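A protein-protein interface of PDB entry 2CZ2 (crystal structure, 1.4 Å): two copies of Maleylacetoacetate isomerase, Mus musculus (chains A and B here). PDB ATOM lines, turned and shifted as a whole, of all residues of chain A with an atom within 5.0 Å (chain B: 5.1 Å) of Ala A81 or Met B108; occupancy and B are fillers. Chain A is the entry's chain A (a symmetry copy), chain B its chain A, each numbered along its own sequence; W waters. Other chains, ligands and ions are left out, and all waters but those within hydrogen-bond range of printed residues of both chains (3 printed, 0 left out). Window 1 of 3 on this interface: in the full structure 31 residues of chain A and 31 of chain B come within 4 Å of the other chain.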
ATOM      1  N   THR A  75      -9.043  21.224  11.359  1.00  0.00           N
ATOM      2  CA  THR A  75     -10.228  20.379  11.313  1.00  0.00           C
ATOM      3  C   THR A  75     -10.543  19.972  12.739  1.00  0.00           C
ATOM      4  O   THR A  75      -9.697  19.385  13.426  1.00  0.00           O
ATOM      5  CB  THR A  75      -9.985  19.122  10.445  1.00  0.00           C
ATOM      6  OG1 THR A  75      -9.685  19.517   9.109  1.00  0.00           O
ATOM      7  CG2 THR A  75     -11.256  18.240  10.312  1.00  0.00           C
ATOM      8  N   ILE A  76     -11.743  20.316  13.187  1.00  0.00           N
ATOM      9  CA  ILE A  76     -12.197  19.942  14.515  1.00  0.00           C
ATOM     10  C   ILE A  76     -13.371  19.006  14.431  1.00  0.00           C
ATOM     11  O   ILE A  76     -14.305  19.256  13.699  1.00  0.00           O
ATOM     12  CB  ILE A  76     -12.625  21.211  15.302  1.00  0.00           C
ATOM     13  CG1 ILE A  76     -11.617  22.347  15.191  1.00  0.00           C
ATOM     14  CG2 ILE A  76     -12.868  20.867  16.766  1.00  0.00           C
ATOM     15  CD1 ILE A  76     -12.075  23.592  15.840  1.00  0.00           C
ATOM     16  N   VAL A  77     -13.335  17.934  15.215  1.00  0.00           N
ATOM     17  CA  VAL A  77     -14.466  17.037  15.389  1.00  0.00           C
ATOM     18  C   VAL A  77     -14.921  17.115  16.854  1.00  0.00           C
ATOM     19  O   VAL A  77     -14.272  17.799  17.677  1.00  0.00           O
ATOM     20  CB  VAL A  77     -14.144  15.586  14.978  1.00  0.00           C
ATOM     21  CG1 VAL A  77     -13.694  15.527  13.504  1.00  0.00           C
ATOM     22  CG2 VAL A  77     -13.098  14.986  15.831  1.00  0.00           C
ATOM     23  N   GLN A  78     -16.102  16.550  17.118  1.00  0.00           N
ATOM     24  CA  GLN A  78     -16.795  16.574  18.406  1.00  0.00           C
ATOM     25  C   GLN A  78     -17.528  17.909  18.582  1.00  0.00           C
ATOM     26  O   GLN A  78     -16.923  18.962  18.748  1.00  0.00           O
ATOM     27  CB  GLN A  78     -15.874  16.267  19.574  1.00  0.00           C
ATOM     28  CG  GLN A  78     -15.386  14.831  19.601  1.00  0.00           C
ATOM     29  CD  GLN A  78     -16.470  13.874  20.039  1.00  0.00           C
ATOM     30  OE1 GLN A  78     -17.468  14.267  20.691  1.00  0.00           O
ATOM     31  NE2 GLN A  78     -16.285  12.600  19.704  1.00  0.00           N
ATOM     32  N   SER A  79     -18.849  17.859  18.529  1.00  0.00           N
ATOM     33  CA  SER A  79     -19.643  19.062  18.513  1.00  0.00           C
ATOM     34  C   SER A  79     -19.354  19.998  19.710  1.00  0.00           C
ATOM     35  O   SER A  79     -19.321  21.213  19.537  1.00  0.00           O
ATOM     36  CB  SER A  79     -21.130  18.750  18.428  1.00  0.00           C
ATOM     37  OG  SER A  79     -21.535  18.039  19.543  1.00  0.00           O
ATOM     38  N   LEU A  80     -19.149  19.461  20.913  1.00  0.00           N
ATOM     39  CA  LEU A  80     -18.879  20.328  22.039  1.00  0.00           C
ATOM     40  C   LEU A  80     -17.489  20.921  21.978  1.00  0.00           C
ATOM     41  O   LEU A  80     -17.309  22.070  22.334  1.00  0.00           O
ATOM     42  CB  LEU A  80     -19.129  19.625  23.358  1.00  0.00           C
ATOM     43  CG  LEU A  80     -20.597  19.587  23.790  1.00  0.00           C
ATOM     44  CD1 LEU A  80     -21.520  19.003  22.776  1.00  0.00           C
ATOM     45  CD2 LEU A  80     -20.693  18.841  25.102  1.00  0.00           C
ATOM     46  N   ALA A  81     -16.524  20.180  21.436  1.00  0.00           N
ATOM     47  CA  ALA A  81     -15.202  20.742  21.245  1.00  0.00           C
ATOM     48  C   ALA A  81     -15.215  21.882  20.211  1.00  0.00           C
ATOM     49  O   ALA A  81     -14.555  22.934  20.383  1.00  0.00           O
ATOM     50  CB  ALA A  81     -14.235  19.645  20.830  1.00  0.00           C
ATOM     51  N   ILE A  82     -15.965  21.669  19.134  1.00  0.00           N
ATOM     52  CA  ILE A  82     -16.212  22.710  18.133  1.00  0.00           C
ATOM     53  C   ILE A  82     -16.836  23.947  18.757  1.00  0.00           C
ATOM     54  O   ILE A  82     -16.358  25.046  18.557  1.00  0.00           O
ATOM     55  CB  ILE A  82     -17.119  22.171  17.016  1.00  0.00           C
ATOM     56  CG1 ILE A  82     -16.386  21.085  16.228  1.00  0.00           C
ATOM     57  CG2 ILE A  82     -17.563  23.322  16.094  1.00  0.00           C
ATOM     58  CD1 ILE A  82     -17.276  20.232  15.389  1.00  0.00           C
ATOM     59  N   MET A  83     -17.893  23.758  19.533  1.00  0.00           N
ATOM     60  CA  MET A  83     -18.598  24.893  20.119  1.00  0.00           C
ATOM     61  C   MET A  83     -17.723  25.644  21.122  1.00  0.00           C
ATOM     62  O   MET A  83     -17.740  26.848  21.145  1.00  0.00           O
ATOM     63  CB  MET A  83     -19.939  24.443  20.723  1.00  0.00           C
ATOM     64  CG  MET A  83     -20.931  24.049  19.674  1.00  0.00           C
ATOM     65  SD  MET A  83     -22.722  23.795  20.342  1.00  0.00           S
ATOM     66  CE  MET A  83     -22.455  22.295  21.250  1.00  0.00           C
ATOM     67  N   GLU A  84     -16.937  24.932  21.917  1.00  0.00           N
ATOM     68  CA  GLU A  84     -15.977  25.600  22.817  1.00  0.00           C
ATOM     69  C   GLU A  84     -14.917  26.410  22.039  1.00  0.00           C
ATOM     70  O   GLU A  84     -14.518  27.514  22.467  1.00  0.00           O
ATOM     71  CB  GLU A  84     -15.287  24.609  23.763  1.00  0.00           C
ATOM     72  CG  GLU A  84     -16.291  23.850  24.651  1.00  0.00           C
ATOM     73  CD  GLU A  84     -16.337  24.346  26.097  1.00  0.00           C
ATOM     74  OE1 GLU A  84     -15.748  25.368  26.446  1.00  0.00           O
ATOM     75  OE2 GLU A  84     -16.980  23.724  26.937  1.00  0.00           O
ATOM     76  N   TYR A  85     -14.463  25.880  20.900  1.00  0.00           N
ATOM     77  CA  TYR A  85     -13.544  26.627  20.033  1.00  0.00           C
ATOM     78  C   TYR A  85     -14.185  27.900  19.494  1.00  0.00           C
ATOM     79  O   TYR A  85     -13.607  28.960  19.525  1.00  0.00           O
ATOM     80  CB  TYR A  85     -13.053  25.737  18.886  1.00  0.00           C
ATOM     81  CG  TYR A  85     -12.097  26.452  17.985  1.00  0.00           C
ATOM     82  CD1 TYR A  85     -10.747  26.571  18.315  1.00  0.00           C
ATOM     83  CD2 TYR A  85     -12.522  27.049  16.807  1.00  0.00           C
ATOM     84  CE1 TYR A  85      -9.879  27.235  17.503  1.00  0.00           C
ATOM     85  CE2 TYR A  85     -11.628  27.693  15.969  1.00  0.00           C
ATOM     86  CZ  TYR A  85     -10.317  27.819  16.342  1.00  0.00           C
ATOM     87  OH  TYR A  85      -9.390  28.468  15.537  1.00  0.00           O
ATOM     88  N   ARG B 103      -6.269  23.558  22.344  1.00  0.00           N
ATOM     89  CA  ARG B 103      -7.360  23.271  23.293  1.00  0.00           C
ATOM     90  C   ARG B 103      -8.456  22.439  22.618  1.00  0.00           C
ATOM     91  O   ARG B 103      -9.020  21.511  23.210  1.00  0.00           O
ATOM     92  CB  ARG B 103      -7.956  24.539  23.829  1.00  0.00           C
ATOM     93  CG  ARG B 103      -7.060  25.296  24.754  1.00  0.00           C
ATOM     94  CD  ARG B 103      -7.432  26.747  25.002  1.00  0.00           C
ATOM     95  NE  ARG B 103      -8.620  26.853  25.828  1.00  0.00           N
ATOM     96  CZ  ARG B 103      -8.610  26.899  27.159  1.00  0.00           C
ATOM     97  NH1 ARG B 103      -7.478  26.750  27.844  1.00  0.00           N
ATOM     98  NH2 ARG B 103      -9.752  27.046  27.819  1.00  0.00           N
ATOM     99  N   ALA B 104      -8.785  22.783  21.379  1.00  0.00           N
ATOM    100  CA  ALA B 104      -9.794  22.011  20.637  1.00  0.00           C
ATOM    101  C   ALA B 104      -9.405  20.567  20.458  1.00  0.00           C
ATOM    102  O   ALA B 104     -10.244  19.676  20.538  1.00  0.00           O
ATOM    103  CB  ALA B 104     -10.037  22.635  19.273  1.00  0.00           C
ATOM    104  N   ILE B 105      -8.127  20.307  20.209  1.00  0.00           N
ATOM    105  CA  ILE B 105      -7.677  18.927  20.050  1.00  0.00           C
ATOM    106  C   ILE B 105      -7.790  18.159  21.372  1.00  0.00           C
ATOM    107  O   ILE B 105      -8.225  16.996  21.408  1.00  0.00           O
ATOM    108  CB  ILE B 105      -6.228  18.893  19.560  1.00  0.00           C
ATOM    109  CG1 ILE B 105      -6.095  19.628  18.231  1.00  0.00           C
ATOM    110  CG2 ILE B 105      -5.741  17.422  19.422  1.00  0.00           C
ATOM    111  CD1 ILE B 105      -4.662  19.695  17.760  1.00  0.00           C
ATOM    112  N   VAL B 106      -7.396  18.795  22.473  1.00  0.00           N
ATOM    113  CA  VAL B 106      -7.520  18.158  23.779  1.00  0.00           C
ATOM    114  C   VAL B 106      -8.973  17.854  24.082  1.00  0.00           C
ATOM    115  O   VAL B 106      -9.315  16.779  24.557  1.00  0.00           O
ATOM    116  CB  VAL B 106      -6.964  19.060  24.919  1.00  0.00           C
ATOM    117  CG1 VAL B 106      -7.326  18.449  26.288  1.00  0.00           C
ATOM    118  CG2 VAL B 106      -5.456  19.212  24.778  1.00  0.00           C
ATOM    119  N   ARG B 107      -9.852  18.809  23.803  1.00  0.00           N
ATOM    120  CA  ARG B 107     -11.255  18.579  24.081  1.00  0.00           C
ATOM    121  C   ARG B 107     -11.840  17.506  23.127  1.00  0.00           C
ATOM    122  O   ARG B 107     -12.682  16.718  23.514  1.00  0.00           O
ATOM    123  CB  ARG B 107     -12.072  19.850  23.980  1.00  0.00           C
ATOM    124  CG  ARG B 107     -11.813  20.890  25.029  1.00  0.00           C
ATOM    125  CD  ARG B 107     -12.986  21.816  25.177  1.00  0.00           C
ATOM    126  NE  ARG B 107     -12.850  22.761  26.286  1.00  0.00           N
ATOM    127  CZ  ARG B 107     -12.400  23.999  26.212  1.00  0.00           C
ATOM    128  NH1 ARG B 107     -12.009  24.555  25.064  1.00  0.00           N
ATOM    129  NH2 ARG B 107     -12.407  24.699  27.336  1.00  0.00           N
ATOM    130  N   MET B 108     -11.381  17.472  21.886  1.00  0.00           N
ATOM    131  CA  MET B 108     -11.871  16.484  20.921  1.00  0.00           C
ATOM    132  C   MET B 108     -11.596  15.063  21.416  1.00  0.00           C
ATOM    133  O   MET B 108     -12.435  14.189  21.332  1.00  0.00           O
ATOM    134  CB  MET B 108     -11.109  16.637  19.593  1.00  0.00           C
ATOM    135  CG  MET B 108     -11.512  17.650  18.660  1.00  0.00           C
ATOM    136  SD  MET B 108     -10.214  17.547  17.203  1.00  0.00           S
ATOM    137  CE  MET B 108     -10.328  15.849  16.674  1.00  0.00           C
ATOM    138  N   ILE B 109     -10.367  14.844  21.872  1.00  0.00           N
ATOM    139  CA  ILE B 109      -9.961  13.526  22.334  1.00  0.00           C
ATOM    140  C   ILE B 109     -10.691  13.155  23.635  1.00  0.00           C
ATOM    141  O   ILE B 109     -11.174  12.028  23.811  1.00  0.00           O
ATOM    142  CB  ILE B 109      -8.450  13.450  22.514  1.00  0.00           C
ATOM    143  CG1 ILE B 109      -7.748  13.511  21.132  1.00  0.00           C
ATOM    144  CG2 ILE B 109      -8.038  12.177  23.236  1.00  0.00           C
ATOM    145  CD1 ILE B 109      -6.313  13.838  21.236  1.00  0.00           C
ATOM    146  N   SER B 110     -10.824  14.130  24.515  1.00  0.00           N
ATOM    147  CA  SER B 110     -11.535  13.916  25.773  1.00  0.00           C
ATOM    148  C   SER B 110     -12.983  13.517  25.501  1.00  0.00           C
ATOM    149  O   SER B 110     -13.461  12.560  26.085  1.00  0.00           O
ATOM    150  CB  SER B 110     -11.435  15.153  26.692  1.00  0.00           C
ATOM    151  OG  SER B 110     -10.091  15.549  26.983  1.00  0.00           O
ATOM    152  N   ASP B 111     -13.634  14.187  24.555  1.00  0.00           N
ATOM    153  CA  ASP B 111     -15.016  13.896  24.184  1.00  0.00           C
ATOM    154  C   ASP B 111     -15.153  12.570  23.420  1.00  0.00           C
ATOM    155  O   ASP B 111     -16.113  11.859  23.616  1.00  0.00           O
ATOM    156  CB  ASP B 111     -15.607  15.018  23.333  1.00  0.00           C
ATOM    157  CG  ASP B 111     -15.844  16.305  24.067  1.00  0.00           C
ATOM    158  OD1 ASP B 111     -15.750  16.373  25.330  1.00  0.00           O
ATOM    159  OD2 ASP B 111     -16.180  17.326  23.393  1.00  0.00           O
ATOM    160  N   LEU B 112     -14.176  12.217  22.571  1.00  0.00           N
ATOM    161  CA  LEU B 112     -14.176  10.947  21.899  1.00  0.00           C
ATOM    162  C   LEU B 112     -14.301   9.850  22.972  1.00  0.00           C
ATOM    163  O   LEU B 112     -15.113   8.937  22.879  1.00  0.00           O
ATOM    164  CB  LEU B 112     -12.884  10.771  21.079  1.00  0.00           C
ATOM    165  CG  LEU B 112     -12.757   9.540  20.201  1.00  0.00           C
ATOM    166  CD1 LEU B 112     -11.770   9.763  19.055  1.00  0.00           C
ATOM    167  CD2 LEU B 112     -12.327   8.315  21.017  1.00  0.00           C
ATOM    168  N   ILE B 152      -5.956   9.054  15.406  1.00  0.00           N
ATOM    169  CA  ILE B 152      -5.853  10.466  15.745  1.00  0.00           C
ATOM    170  C   ILE B 152      -4.548  10.782  16.453  1.00  0.00           C
ATOM    171  O   ILE B 152      -3.889  11.777  16.124  1.00  0.00           O
ATOM    172  CB  ILE B 152      -7.077  10.912  16.606  1.00  0.00           C
ATOM    173  CG1 ILE B 152      -8.345  10.910  15.727  1.00  0.00           C
ATOM    174  CG2 ILE B 152      -6.845  12.286  17.219  1.00  0.00           C
ATOM    175  CD1 ILE B 152      -9.695  10.815  16.483  1.00  0.00           C
HETATM  176  O   HOH W   1     -18.670  16.593  21.753  1.00  0.00           O
HETATM  177  O   HOH W   2     -15.693  19.642  24.625  1.00  0.00           O
HETATM  178  O   HOH W   3     -12.240  23.553  22.215  1.00  0.00           O
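Met B108 touches four residues of chain A. Printed residues of chain A within 4 Å of Leu B112: Gln A78. Printed residues of chain A within 4 Å of Arg B107: Ala A81 (3.8 Å) and Glu A84 (3.5 Å). Of the printed residues of chain B, Gln A78 touches Met B108, Asp B111 and Leu B112. Ile B152 touches none of the printed residues of chain A. Ser B110 touches none of the printed residues of chain A.
Water W2 lies within hydrogen-bond range of the side-chain carboxylate (OD2) of Asp B111 (2.7 Å) and the backbone NH (N) of Ala A81 (3.3 Å). Water W1 lies within hydrogen-bond range of OE1 of Gln A78 (2.8 Å), N of Leu A80 (3.0 Å), OD2 of Asp B111 (3.1 Å) and N of Ser A79 (3.5 Å). Water W3 lies within hydrogen-bond range of O of Ala A81, NH1 of Arg B107 and N of Tyr A85.
The guanidinium group of Arg B107 is in salt-bridge range of the side-chain carboxylate of Glu A84, 3.5 Å away. N of Val A77 is in hydrogen-bond range of SD of Met B108, at 3.7 Å. The backbone NH (N) of Ala A81 sits at hydrogen-bond distance from the side-chain carboxylate (OD2) of Asp B111.
Among the printed residues, merely in contact across the chains: Gln A78 with Asp B111 (3.3 Å), Gln A78 with Leu B112 (3.5 Å), Gln A78 with Met B108 (3.5 Å), Ala A81 with Met B108 (3.7 Å), Leu A80 with Asp B111 (3.7 Å), Ala A81 with Arg B107 (3.8 Å) and Ile A76 with Met B108 (3.97 Å).
Of the 11 printed residues of chain A, 6 touch a printed residue of chain B. Printed residues of chain A that touch a printed residue of chain B: Ile A76, Val A77, Gln A78, Leu A80, Ala A81 and Glu A84. Along chain A the printed residues that touch a printed residue of chain B span positions 76 to 84. Printed residues of chain B that touch a printed residue of chain A: Arg B107, Met B108, Asp B111 and Leu B112. Hydrophobic or aromatic side chains of chain B within 4 Å of the printed part of chain A: Met B108. Among the printed residues, 10 pairs touch across the chains. Among the printed residues, Asp or Glu carboxylates within 4 Å of a Lys or Arg side-chain nitrogen of the other chain: Glu A84 with Arg B107 (3.5 Å).
No position is printed for both chains. Of the 10 pairs that touch across the chains among the printed residues, none has its exchanged pair printed and touching as well.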
